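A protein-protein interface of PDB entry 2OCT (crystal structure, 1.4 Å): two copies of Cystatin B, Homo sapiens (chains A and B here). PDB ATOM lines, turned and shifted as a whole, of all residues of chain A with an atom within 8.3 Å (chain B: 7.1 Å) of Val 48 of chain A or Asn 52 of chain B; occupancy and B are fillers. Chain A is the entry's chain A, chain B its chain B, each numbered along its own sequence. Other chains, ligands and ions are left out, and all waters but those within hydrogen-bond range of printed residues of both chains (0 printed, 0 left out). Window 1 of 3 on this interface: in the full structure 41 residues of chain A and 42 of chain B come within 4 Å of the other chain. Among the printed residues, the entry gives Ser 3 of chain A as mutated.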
ATOM      1  N   MET A   2      -4.630  13.143  11.702  1.00  0.00           N
ATOM      2  CA  MET A   2      -3.469  13.817  11.123  1.00  0.00           C
ATOM      3  C   MET A   2      -3.411  15.028  11.901  1.00  0.00           C
ATOM      4  O   MET A   2      -3.107  16.091  11.361  1.00  0.00           O
ATOM      5  CB  MET A   2      -3.764  14.327   9.711  1.00  0.00           C
ATOM      6  CG  MET A   2      -4.264  15.764   9.663  1.00  0.00           C
ATOM      7  SD  MET A   2      -5.017  16.147   8.068  1.00  0.00           S
ATOM      8  CE  MET A   2      -6.398  17.166   8.617  1.00  0.00           C
ATOM      9  N   SER A   3      -3.665  15.064  13.204  1.00  0.00           N
ATOM     10  CA  SER A   3      -3.649  16.205  14.098  1.00  0.00           C
ATOM     11  C   SER A   3      -3.321  17.577  13.531  1.00  0.00           C
ATOM     12  O   SER A   3      -2.948  17.722  12.369  1.00  0.00           O
ATOM     13  N   GLY A   4      -3.446  18.612  14.356  1.00  0.00           N
ATOM     14  CA  GLY A   4      -3.021  19.957  13.945  1.00  0.00           C
ATOM     15  C   GLY A   4      -1.845  20.205  14.882  1.00  0.00           C
ATOM     16  O   GLY A   4      -1.149  21.215  14.875  1.00  0.00           O
ATOM     17  N   ALA A   5      -1.647  19.185  15.726  1.00  0.00           N
ATOM     18  CA  ALA A   5      -0.511  19.251  16.647  1.00  0.00           C
ATOM     19  C   ALA A   5       0.771  19.223  15.836  1.00  0.00           C
ATOM     20  O   ALA A   5       0.855  18.501  14.846  1.00  0.00           O
ATOM     21  CB  ALA A   5      -0.577  18.117  17.653  1.00  0.00           C
ATOM     22  N   PRO A   6       1.779  19.988  16.204  1.00  0.00           N
ATOM     23  CA  PRO A   6       3.049  19.876  15.475  1.00  0.00           C
ATOM     24  C   PRO A   6       3.627  18.478  15.660  1.00  0.00           C
ATOM     25  O   PRO A   6       3.600  17.893  16.741  1.00  0.00           O
ATOM     26  CB  PRO A   6       3.948  20.915  16.134  1.00  0.00           C
ATOM     27  CG  PRO A   6       3.085  21.787  16.976  1.00  0.00           C
ATOM     28  CD  PRO A   6       1.841  20.996  17.274  1.00  0.00           C
ATOM     29  N   SER A   7       4.169  17.912  14.587  1.00  0.00           N
ATOM     30  CA  SER A   7       4.785  16.601  14.679  1.00  0.00           C
ATOM     31  C   SER A   7       5.938  16.620  15.679  1.00  0.00           C
ATOM     32  O   SER A   7       6.337  17.673  16.171  1.00  0.00           O
ATOM     33  CB  SER A   7       5.317  16.158  13.313  1.00  0.00           C
ATOM     34  OG  SER A   7       6.527  16.840  13.025  1.00  0.00           O
ATOM     35  N   ILE A  19      13.047  23.106   0.511  1.00  0.00           N
ATOM     36  CA  ILE A  19      12.348  24.265   1.096  1.00  0.00           C
ATOM     37  C   ILE A  19      13.319  25.339   1.564  1.00  0.00           C
ATOM     38  O   ILE A  19      13.165  26.543   1.270  1.00  0.00           O
ATOM     39  CB  ILE A  19      11.467  23.792   2.259  1.00  0.00           C
ATOM     40  CG1 ILE A  19      10.304  22.893   1.817  1.00  0.00           C
ATOM     41  CG2 ILE A  19      10.923  24.960   3.063  1.00  0.00           C
ATOM     42  CD1 ILE A  19       9.539  22.281   2.975  1.00  0.00           C
ATOM     43  N   PHE A  43      13.123  19.237  11.204  1.00  0.00           N
ATOM     44  CA  PHE A  43      11.881  19.987  11.085  1.00  0.00           C
ATOM     45  C   PHE A  43      10.770  19.363  11.904  1.00  0.00           C
ATOM     46  O   PHE A  43      10.805  18.196  12.299  1.00  0.00           O
ATOM     47  CB  PHE A  43      11.468  20.054   9.607  1.00  0.00           C
ATOM     48  CG  PHE A  43      10.938  18.753   9.007  1.00  0.00           C
ATOM     49  CD1 PHE A  43      11.794  17.798   8.493  1.00  0.00           C
ATOM     50  CD2 PHE A  43       9.552  18.488   8.943  1.00  0.00           C
ATOM     51  CE1 PHE A  43      11.327  16.614   7.940  1.00  0.00           C
ATOM     52  CE2 PHE A  43       9.073  17.311   8.427  1.00  0.00           C
ATOM     53  CZ  PHE A  43       9.969  16.353   7.944  1.00  0.00           C
ATOM     54  N   LYS A  44       9.754  20.169  12.149  1.00  0.00           N
ATOM     55  CA  LYS A  44       8.428  19.754  12.583  1.00  0.00           C
ATOM     56  C   LYS A  44       7.399  20.172  11.539  1.00  0.00           C
ATOM     57  O   LYS A  44       7.564  21.225  10.971  1.00  0.00           O
ATOM     58  CB  LYS A  44       8.078  20.411  13.918  1.00  0.00           C
ATOM     59  CG  LYS A  44       8.933  19.905  15.083  1.00  0.00           C
ATOM     60  CD  LYS A  44       8.405  20.451  16.406  1.00  0.00           C
ATOM     61  CE  LYS A  44       9.304  19.956  17.533  1.00  0.00           C
ATOM     62  NZ  LYS A  44       8.755  18.819  18.295  1.00  0.00           N
ATOM     63  N   SER A  45       6.359  19.394  11.291  1.00  0.00           N
ATOM     64  CA  SER A  45       5.262  19.767  10.417  1.00  0.00           C
ATOM     65  C   SER A  45       3.995  19.962  11.257  1.00  0.00           C
ATOM     66  O   SER A  45       3.804  19.312  12.296  1.00  0.00           O
ATOM     67  CB  SER A  45       4.996  18.749   9.302  1.00  0.00           C
ATOM     68  OG  SER A  45       4.663  17.468   9.755  1.00  0.00           O
ATOM     69  N   GLN A  46       3.141  20.848  10.769  1.00  0.00           N
ATOM     70  CA  GLN A  46       1.852  21.121  11.383  1.00  0.00           C
ATOM     71  C   GLN A  46       0.817  21.304  10.301  1.00  0.00           C
ATOM     72  O   GLN A  46       0.937  22.167   9.444  1.00  0.00           O
ATOM     73  CB  GLN A  46       1.978  22.403  12.230  1.00  0.00           C
ATOM     74  CG  GLN A  46       0.686  22.944  12.832  1.00  0.00           C
ATOM     75  CD  GLN A  46       0.866  24.348  13.430  1.00  0.00           C
ATOM     76  OE1 GLN A  46       0.481  24.633  14.569  1.00  0.00           O
ATOM     77  NE2 GLN A  46       1.468  25.283  12.693  1.00  0.00           N
ATOM     78  N   VAL A  47      -0.217  20.469  10.320  1.00  0.00           N
ATOM     79  CA  VAL A  47      -1.291  20.577   9.356  1.00  0.00           C
ATOM     80  C   VAL A  47      -2.112  21.800   9.763  1.00  0.00           C
ATOM     81  O   VAL A  47      -2.418  21.962  10.961  1.00  0.00           O
ATOM     82  CB  VAL A  47      -2.181  19.304   9.355  1.00  0.00           C
ATOM     83  CG1 VAL A  47      -3.417  19.533   8.536  1.00  0.00           C
ATOM     84  CG2 VAL A  47      -1.428  18.066   8.825  1.00  0.00           C
ATOM     85  N   VAL A  48      -2.431  22.632   8.784  1.00  0.00           N
ATOM     86  CA  VAL A  48      -3.279  23.781   8.950  1.00  0.00           C
ATOM     87  C   VAL A  48      -4.447  23.664   7.983  1.00  0.00           C
ATOM     88  O   VAL A  48      -4.222  23.498   6.783  1.00  0.00           O
ATOM     89  CB  VAL A  48      -2.490  25.076   8.667  1.00  0.00           C
ATOM     90  CG1 VAL A  48      -3.350  26.312   8.851  1.00  0.00           C
ATOM     91  CG2 VAL A  48      -1.281  25.182   9.603  1.00  0.00           C
ATOM     92  N   ALA A  49      -5.664  23.757   8.510  1.00  0.00           N
ATOM     93  CA  ALA A  49      -6.820  23.712   7.603  1.00  0.00           C
ATOM     94  C   ALA A  49      -7.968  24.454   8.272  1.00  0.00           C
ATOM     95  O   ALA A  49      -8.428  24.088   9.361  1.00  0.00           O
ATOM     96  CB  ALA A  49      -7.210  22.283   7.254  1.00  0.00           C
ATOM     97  N   GLY A  50      -8.431  25.524   7.622  1.00  0.00           N
ATOM     98  CA  GLY A  50      -9.480  26.346   8.272  1.00  0.00           C
ATOM     99  C   GLY A  50      -9.755  27.567   7.428  1.00  0.00           C
ATOM    100  O   GLY A  50      -9.429  27.579   6.234  1.00  0.00           O
ATOM    101  N   THR A  51     -10.359  28.569   8.017  1.00  0.00           N
ATOM    102  CA  THR A  51     -10.727  29.769   7.307  1.00  0.00           C
ATOM    103  C   THR A  51     -10.047  30.990   7.944  1.00  0.00           C
ATOM    104  O   THR A  51     -10.196  31.219   9.142  1.00  0.00           O
ATOM    105  CB  THR A  51     -12.264  29.991   7.361  1.00  0.00           C
ATOM    106  OG1 THR A  51     -12.945  28.783   6.956  1.00  0.00           O
ATOM    107  CG2 THR A  51     -12.668  31.107   6.417  1.00  0.00           C
ATOM    108  N   ASN A  52      -9.355  31.752   7.102  1.00  0.00           N
ATOM    109  CA  ASN A  52      -8.890  33.075   7.514  1.00  0.00           C
ATOM    110  C   ASN A  52     -10.029  34.061   7.278  1.00  0.00           C
ATOM    111  O   ASN A  52     -10.730  33.977   6.265  1.00  0.00           O
ATOM    112  CB  ASN A  52      -7.682  33.517   6.694  1.00  0.00           C
ATOM    113  CG  ASN A  52      -6.314  33.225   7.275  1.00  0.00           C
ATOM    114  OD1 ASN A  52      -6.209  32.910   8.467  1.00  0.00           O
ATOM    115  ND2 ASN A  52      -5.292  33.301   6.432  1.00  0.00           N
ATOM    116  N   PHE A  70      -8.071  33.462  12.474  1.00  0.00           N
ATOM    117  CA  PHE A  70      -8.156  32.141  11.891  1.00  0.00           C
ATOM    118  C   PHE A  70      -9.093  31.242  12.677  1.00  0.00           C
ATOM    119  O   PHE A  70      -9.059  31.219  13.930  1.00  0.00           O
ATOM    120  CB  PHE A  70      -6.761  31.509  11.843  1.00  0.00           C
ATOM    121  CG  PHE A  70      -6.733  30.099  11.266  1.00  0.00           C
ATOM    122  CD1 PHE A  70      -6.918  29.884   9.908  1.00  0.00           C
ATOM    123  CD2 PHE A  70      -6.530  28.994  12.095  1.00  0.00           C
ATOM    124  CE1 PHE A  70      -6.866  28.584   9.390  1.00  0.00           C
ATOM    125  CE2 PHE A  70      -6.478  27.700  11.589  1.00  0.00           C
ATOM    126  CZ  PHE A  70      -6.672  27.520  10.226  1.00  0.00           C
ATOM    127  N   GLN A  71      -9.914  30.524  11.903  1.00  0.00           N
ATOM    128  CA  GLN A  71     -10.841  29.532  12.476  1.00  0.00           C
ATOM    129  C   GLN A  71     -10.461  28.158  11.957  1.00  0.00           C
ATOM    130  O   GLN A  71     -10.613  27.905  10.759  1.00  0.00           O
ATOM    131  CB  GLN A  71     -12.282  29.902  12.112  1.00  0.00           C
ATOM    132  CG  GLN A  71     -13.369  29.079  12.808  1.00  0.00           C
ATOM    133  CD  GLN A  71     -14.777  29.511  12.454  1.00  0.00           C
ATOM    134  OE1 GLN A  71     -14.936  30.369  11.572  1.00  0.00           O
ATOM    135  NE2 GLN A  71     -15.806  28.960  13.099  1.00  0.00           N
ATOM    136  N   SER A  72      -9.966  27.275  12.820  1.00  0.00           N
ATOM    137  CA  SER A  72      -9.602  25.933  12.356  1.00  0.00           C
ATOM    138  C   SER A  72     -10.808  25.064  12.048  1.00  0.00           C
ATOM    139  O   SER A  72     -11.855  25.210  12.689  1.00  0.00           O
ATOM    140  CB  SER A  72      -8.786  25.244  13.481  1.00  0.00           C
ATOM    141  OG  SER A  72      -8.342  23.963  13.058  1.00  0.00           O
ATOM    142  N   LEU A  73     -10.679  24.125  11.125  1.00  0.00           N
ATOM    143  CA  LEU A  73     -11.625  22.995  11.090  1.00  0.00           C
ATOM    144  C   LEU A  73     -11.627  22.295  12.430  1.00  0.00           C
ATOM    145  O   LEU A  73     -10.642  22.437  13.211  1.00  0.00           O
ATOM    146  CB  LEU A  73     -11.239  22.041   9.963  1.00  0.00           C
ATOM    147  CG  LEU A  73     -11.604  22.502   8.544  1.00  0.00           C
ATOM    148  CD1 LEU A  73     -10.956  21.581   7.504  1.00  0.00           C
ATOM    149  CD2 LEU A  73     -13.119  22.588   8.343  1.00  0.00           C
ATOM    150  N   VAL B  48      -7.717  28.264   3.951  1.00  0.00           N
ATOM    151  CA  VAL B  48      -6.326  27.917   4.165  1.00  0.00           C
ATOM    152  C   VAL B  48      -6.211  26.410   4.343  1.00  0.00           C
ATOM    153  O   VAL B  48      -6.931  25.845   5.168  1.00  0.00           O
ATOM    154  CB  VAL B  48      -5.755  28.574   5.446  1.00  0.00           C
ATOM    155  CG1 VAL B  48      -4.260  28.221   5.591  1.00  0.00           C
ATOM    156  CG2 VAL B  48      -5.989  30.075   5.423  1.00  0.00           C
ATOM    157  N   ALA B  49      -5.345  25.739   3.598  1.00  0.00           N
ATOM    158  CA  ALA B  49      -5.190  24.292   3.814  1.00  0.00           C
ATOM    159  C   ALA B  49      -3.805  23.931   3.294  1.00  0.00           C
ATOM    160  O   ALA B  49      -3.489  24.098   2.110  1.00  0.00           O
ATOM    161  CB  ALA B  49      -6.292  23.519   3.094  1.00  0.00           C
ATOM    162  N   GLY B  50      -2.948  23.497   4.212  1.00  0.00           N
ATOM    163  CA  GLY B  50      -1.590  23.149   3.853  1.00  0.00           C
ATOM    164  C   GLY B  50      -0.805  22.705   5.080  1.00  0.00           C
ATOM    165  O   GLY B  50      -1.374  22.335   6.111  1.00  0.00           O
ATOM    166  N   THR B  51       0.519  22.724   4.930  1.00  0.00           N
ATOM    167  CA  THR B  51       1.424  22.310   5.970  1.00  0.00           C
ATOM    168  C   THR B  51       2.298  23.487   6.393  1.00  0.00           C
ATOM    169  O   THR B  51       2.890  24.108   5.496  1.00  0.00           O
ATOM    170  CB  THR B  51       2.366  21.203   5.454  1.00  0.00           C
ATOM    171  OG1 THR B  51       1.559  20.143   4.896  1.00  0.00           O
ATOM    172  CG2 THR B  51       3.149  20.610   6.601  1.00  0.00           C
ATOM    173  N   ASN B  52       2.370  23.725   7.677  1.00  0.00           N
ATOM    174  CA  ASN B  52       3.405  24.639   8.201  1.00  0.00           C
ATOM    175  C   ASN B  52       4.652  23.818   8.483  1.00  0.00           C
ATOM    176  O   ASN B  52       4.552  22.756   9.124  1.00  0.00           O
ATOM    177  CB  ASN B  52       2.903  25.310   9.474  1.00  0.00           C
ATOM    178  CG  ASN B  52       2.412  26.726   9.301  1.00  0.00           C
ATOM    179  OD1 ASN B  52       2.592  27.387   8.276  1.00  0.00           O
ATOM    180  ND2 ASN B  52       1.736  27.182  10.361  1.00  0.00           N
ATOM    181  N   TYR B  53       5.804  24.272   8.059  1.00  0.00           N
ATOM    182  CA  TYR B  53       7.080  23.672   8.461  1.00  0.00           C
ATOM    183  C   TYR B  53       7.851  24.601   9.379  1.00  0.00           C
ATOM    184  O   TYR B  53       7.990  25.789   9.082  1.00  0.00           O
ATOM    185  CB  TYR B  53       7.890  23.317   7.201  1.00  0.00           C
ATOM    186  CG  TYR B  53       7.307  22.154   6.439  1.00  0.00           C
ATOM    187  CD1 TYR B  53       7.502  20.858   6.922  1.00  0.00           C
ATOM    188  CD2 TYR B  53       6.586  22.311   5.267  1.00  0.00           C
ATOM    189  CE1 TYR B  53       7.007  19.707   6.298  1.00  0.00           C
ATOM    190  CE2 TYR B  53       6.074  21.167   4.626  1.00  0.00           C
ATOM    191  CZ  TYR B  53       6.292  19.916   5.141  1.00  0.00           C
ATOM    192  OH  TYR B  53       5.774  18.815   4.489  1.00  0.00           O
ATOM    193  N   PHE B  54       8.334  24.022  10.479  1.00  0.00           N
ATOM    194  CA  PHE B  54       9.278  24.693  11.356  1.00  0.00           C
ATOM    195  C   PHE B  54      10.618  24.024  11.147  1.00  0.00           C
ATOM    196  O   PHE B  54      10.643  22.834  11.474  1.00  0.00           O
ATOM    197  CB  PHE B  54       8.825  24.564  12.812  1.00  0.00           C
ATOM    198  CG  PHE B  54       7.519  25.320  13.023  1.00  0.00           C
ATOM    199  CD1 PHE B  54       7.535  26.649  13.400  1.00  0.00           C
ATOM    200  CD2 PHE B  54       6.298  24.699  12.834  1.00  0.00           C
ATOM    201  CE1 PHE B  54       6.335  27.326  13.563  1.00  0.00           C
ATOM    202  CE2 PHE B  54       5.106  25.384  13.012  1.00  0.00           C
ATOM    203  CZ  PHE B  54       5.130  26.721  13.381  1.00  0.00           C
ATOM    204  N   ILE B  55      11.583  24.744  10.626  1.00  0.00           N
ATOM    205  CA  ILE B  55      12.803  24.102  10.124  1.00  0.00           C
ATOM    206  C   ILE B  55      14.036  24.730  10.777  1.00  0.00           C
ATOM    207  O   ILE B  55      14.131  25.955  10.794  1.00  0.00           O
ATOM    208  CB  ILE B  55      12.905  24.230   8.595  1.00  0.00           C
ATOM    209  CG1 ILE B  55      11.646  23.751   7.875  1.00  0.00           C
ATOM    210  CG2 ILE B  55      14.130  23.483   8.068  1.00  0.00           C
ATOM    211  CD1 ILE B  55      11.626  24.037   6.404  1.00  0.00           C
ATOM    212  N   ARG B  68       9.741  29.408   9.745  1.00  0.00           N
ATOM    213  CA  ARG B  68       8.354  28.940   9.659  1.00  0.00           C
ATOM    214  C   ARG B  68       7.900  29.131   8.222  1.00  0.00           C
ATOM    215  O   ARG B  68       7.829  30.299   7.775  1.00  0.00           O
ATOM    216  CB  ARG B  68       7.463  29.743  10.611  1.00  0.00           C
ATOM    217  CG  ARG B  68       5.984  29.545  10.346  1.00  0.00           C
ATOM    218  CD  ARG B  68       5.159  30.476  11.267  1.00  0.00           C
ATOM    219  NE  ARG B  68       3.751  30.383  10.922  1.00  0.00           N
ATOM    220  CZ  ARG B  68       2.703  30.480  11.732  1.00  0.00           C
ATOM    221  NH1 ARG B  68       2.916  30.665  13.027  1.00  0.00           N
ATOM    222  NH2 ARG B  68       1.461  30.376  11.241  1.00  0.00           N
ATOM    223  N   VAL B  69       7.634  28.056   7.508  1.00  0.00           N
ATOM    224  CA  VAL B  69       7.284  28.119   6.100  1.00  0.00           C
ATOM    225  C   VAL B  69       5.952  27.422   5.841  1.00  0.00           C
ATOM    226  O   VAL B  69       5.768  26.297   6.324  1.00  0.00           O
ATOM    227  CB  VAL B  69       8.382  27.441   5.245  1.00  0.00           C
ATOM    228  CG1 VAL B  69       7.939  27.434   3.773  1.00  0.00           C
ATOM    229  CG2 VAL B  69       9.737  28.120   5.419  1.00  0.00           C
ATOM    230  N   PHE B  70       5.062  28.065   5.108  1.00  0.00           N
ATOM    231  CA  PHE B  70       3.778  27.445   4.755  1.00  0.00           C
ATOM    232  C   PHE B  70       3.783  26.968   3.311  1.00  0.00           C
ATOM    233  O   PHE B  70       4.164  27.713   2.404  1.00  0.00           O
ATOM    234  CB  PHE B  70       2.628  28.467   4.910  1.00  0.00           C
ATOM    235  CG  PHE B  70       1.271  27.843   4.607  1.00  0.00           C
ATOM    236  CD1 PHE B  70       0.638  28.202   3.423  1.00  0.00           C
ATOM    237  CD2 PHE B  70       0.662  26.944   5.443  1.00  0.00           C
ATOM    238  CE1 PHE B  70      -0.572  27.669   3.070  1.00  0.00           C
ATOM    239  CE2 PHE B  70      -0.594  26.404   5.117  1.00  0.00           C
ATOM    240  CZ  PHE B  70      -1.212  26.780   3.931  1.00  0.00           C
ATOM    241  N   GLN B  71       3.325  25.715   3.124  1.00  0.00           N
ATOM    242  CA  GLN B  71       3.163  25.076   1.841  1.00  0.00           C
ATOM    243  C   GLN B  71       1.700  24.757   1.631  1.00  0.00           C
ATOM    244  O   GLN B  71       1.175  23.889   2.336  1.00  0.00           O
ATOM    245  CB  GLN B  71       4.060  23.817   1.736  1.00  0.00           C
ATOM    246  CG  GLN B  71       4.042  23.262   0.309  1.00  0.00           C
ATOM    247  CD  GLN B  71       5.031  22.140   0.107  1.00  0.00           C
ATOM    248  OE1 GLN B  71       5.260  21.649  -1.011  1.00  0.00           O
ATOM    249  NE2 GLN B  71       5.639  21.697   1.193  1.00  0.00           N
ATOM    250  N   LEU B  73      -1.808  23.214  -0.011  1.00  0.00           N
ATOM    251  CA  LEU B  73      -2.256  22.178  -0.941  1.00  0.00           C
ATOM    252  C   LEU B  73      -2.372  22.740  -2.351  1.00  0.00           C
ATOM    253  O   LEU B  73      -2.455  23.997  -2.501  1.00  0.00           O
ATOM    254  CB  LEU B  73      -3.594  21.631  -0.466  1.00  0.00           C
ATOM    255  CG  LEU B  73      -3.556  20.684   0.758  1.00  0.00           C
ATOM    256  CD1 LEU B  73      -4.977  20.400   1.258  1.00  0.00           C
ATOM    257  CD2 LEU B  73      -2.823  19.414   0.353  1.00  0.00           C
ATOM    258  N   THR B  81       5.597  29.951   1.250  1.00  0.00           N
ATOM    259  CA  THR B  81       5.661  31.262   1.876  1.00  0.00           C
ATOM    260  C   THR B  81       6.520  31.233   3.120  1.00  0.00           C
ATOM    261  O   THR B  81       6.207  30.488   4.027  1.00  0.00           O
ATOM    262  CB  THR B  81       4.228  31.722   2.253  1.00  0.00           C
ATOM    263  OG1 THR B  81       3.464  31.959   1.072  1.00  0.00           O
ATOM    264  CG2 THR B  81       4.314  33.031   3.038  1.00  0.00           C
ATOM    265  N   SER B  83       6.816  32.586   6.398  1.00  0.00           N
ATOM    266  CA  SER B  83       5.894  33.345   7.240  1.00  0.00           C
ATOM    267  C   SER B  83       6.642  34.089   8.343  1.00  0.00           C
ATOM    268  O   SER B  83       6.271  35.167   8.793  1.00  0.00           O
ATOM    269  CB  SER B  83       4.873  32.437   7.929  1.00  0.00           C
ATOM    270  OG  SER B  83       3.941  31.873   7.042  1.00  0.00           O
ATOM    271  N   TYR B  97       6.938  26.309  18.362  1.00  0.00           N
ATOM    272  CA  TYR B  97       6.037  27.063  17.499  1.00  0.00           C
ATOM    273  C   TYR B  97       6.306  28.556  17.614  1.00  0.00           C
ATOM    274  O   TYR B  97       6.619  29.008  18.733  1.00  0.00           O
ATOM    275  CB  TYR B  97       4.592  26.768  17.925  1.00  0.00           C
ATOM    276  CG  TYR B  97       3.542  27.586  17.210  1.00  0.00           C
ATOM    277  CD1 TYR B  97       3.050  27.155  15.981  1.00  0.00           C
ATOM    278  CD2 TYR B  97       3.032  28.765  17.727  1.00  0.00           C
ATOM    279  CE1 TYR B  97       2.088  27.879  15.296  1.00  0.00           C
ATOM    280  CE2 TYR B  97       2.085  29.485  17.045  1.00  0.00           C
ATOM    281  CZ  TYR B  97       1.606  29.050  15.829  1.00  0.00           C
ATOM    282  OH  TYR B  97       0.645  29.793  15.173  1.00  0.00           O
ATOM    283  N   PHE B  98       6.170  29.294  16.605  1.00  0.00           N
ATOM    284  CA  PHE B  98       6.221  30.755  16.711  1.00  0.00           C
ATOM    285  C   PHE B  98       5.473  31.310  15.489  1.00  0.00           C
ATOM    286  O   PHE B  98       5.235  30.427  14.622  1.00  0.00           O
ATOM    287  CB  PHE B  98       7.642  31.309  16.765  1.00  0.00           C
ATOM    288  CG  PHE B  98       8.503  30.858  15.579  1.00  0.00           C
ATOM    289  CD1 PHE B  98       9.129  29.622  15.583  1.00  0.00           C
ATOM    290  CD2 PHE B  98       8.678  31.669  14.477  1.00  0.00           C
ATOM    291  CE1 PHE B  98       9.897  29.220  14.507  1.00  0.00           C
ATOM    292  CE2 PHE B  98       9.446  31.258  13.392  1.00  0.00           C
ATOM    293  CZ  PHE B  98      10.074  30.019  13.386  1.00  0.00           C
ATOM    294  OXT PHE B  98       5.181  32.428  15.443  1.00  0.00           O
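The backbone NH of Lys 44 of chain A lies within hydrogen-bond range of the backbone carbonyl oxygen of Phe 54 of chain B (2.9 Å). The backbone carbonyl oxygen (O) of Gln 46 of chain A is in hydrogen-bond range of the backbone NH (N) of Asn 52 of chain B (2.8 Å). The backbone carbonyl oxygen (O) of Val 48 of chain A is in hydrogen-bond range of the backbone NH (N) of Gly 50 of chain B (2.9 Å). The backbone NH (N) of Gly 50 of chain A sits at hydrogen-bond distance from the backbone carbonyl oxygen (O) of Val 48 of chain B, at 2.9 Å.
NZ of Lys 44 of chain A lies within hydrogen-bond range of O of Ser 7 of chain A (3.4 Å). The backbone carbonyl oxygen (O) of Ser 45 of chain A is in hydrogen-bond range of the backbone NH (N) of Ser 7 of chain A, 2.7 Å away. O of Ala 49 of chain A sits at hydrogen-bond distance from N of Leu 73 of chain A (2.9 Å). The backbone carbonyl oxygen (O) of Ala 49 of chain B sits at hydrogen-bond distance from the backbone NH (N) of Leu 73 of chain B, 2.8 Å away. The backbone carbonyl oxygen (O) of Thr 51 of chain B lies within hydrogen-bond range of the backbone NH (N) of Gln 71 of chain B (2.9 Å). The side-chain amide nitrogen of Asn 52 of chain B sits close to the guanidinium group of Arg 68 of chain B (3.3 Å).
Among the printed residues, merely in contact across the chains: Phe 43 of chain A with Phe 54 of chain B (3.1 Å), Val 48 of chain A with Ala 49 of chain B (3.2 Å), Ala 49 of chain A with Val 48 of chain B (3.2 Å), Ser 45 of chain A with Asn 52 of chain B (3.3 Å), Asn 52 of chain A with Val 48 of chain B (3.5 Å), Gln 46 of chain A with Thr 51 of chain B (3.5 Å), Ile 19 of chain A with Ile 55 of chain B (3.5 Å), Lys 44 of chain A with Tyr 53 of chain B (3.5 Å), Gln 46 of chain A with Phe 54 of chain B (3.7 Å), Val 47 of chain A with Gly 50 of chain B (3.7 Å), Gln 46 of chain A with Tyr 97 of chain B (3.7 Å), Val 48 of chain A with Asn 52 of chain B (3.7 Å), Phe 43 of chain A with Tyr 53 of chain B (3.7 Å), Ile 19 of chain A with Tyr 53 of chain B (3.7 Å), Ser 45 of chain A with Tyr 53 of chain B (3.7 Å), Ser 45 of chain A with Thr 51 of chain B (3.8 Å), Lys 44 of chain A with Asn 52 of chain B (3.9 Å), Val 48 of chain A with Val 48 of chain B (3.9 Å) and Ile 19 of chain A with Val 69 of chain B (3.9 Å).
Gly 4 of chain A touches none of the printed residues of chain B. Of the printed residues of chain B, Ile 19 of chain A touches Tyr 53, Ile 55 and Val 69. Printed residues of chain B within 4 Å of Lys 44 of chain A: Asn 52, Tyr 53 and Phe 54. Val 48 of chain A touches four residues of chain B. Gly 50 of chain B touches just these residues of chain A: Val 47 (3.7 Å) and Val 48 (2.9 Å). Of chain A, only Lys 44, Ser 45, Gln 46 and Val 48 come within 4 Å of Asn 52 of chain B. Of the printed residues of chain A, Phe 54 of chain B touches Phe 43, Lys 44 and Gln 46. Of the printed residues of chain A, Val 69 of chain B touches Ile 19. The nearest residue of chain B that does not touch Val 48 of chain A is Phe 70 of chain B (4.2 Å).
Of the 17 printed residues of chain B, 10 touch a printed residue of chain A. Hydrophobic or aromatic side chains of chain B within 4 Å of the printed part of chain A: Val 48, Tyr 53, Phe 54, Ile 55, Val 69 and Tyr 97. Among the printed residues, 23 pairs touch across the chains. Among the printed residues, no Asp or Glu carboxylate lies within 4 Å of a Lys or Arg side-chain nitrogen of the other chain.
Val 48 of chain A touches its own counterpart, Val 48 of chain B. Val 48 of chain A touches Ala 49 of chain B, and with the chains exchanged Ala 49 of chain A touches Val 48 of chain B. Val 48 of chain A touches Gly 50 of chain B, and with the chains exchanged Gly 50 of chain A touches Val 48 of chain B. Val 48 of chain A touches Asn 52 of chain B, and with the chains exchanged Asn 52 of chain A touches Val 48 of chain B.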
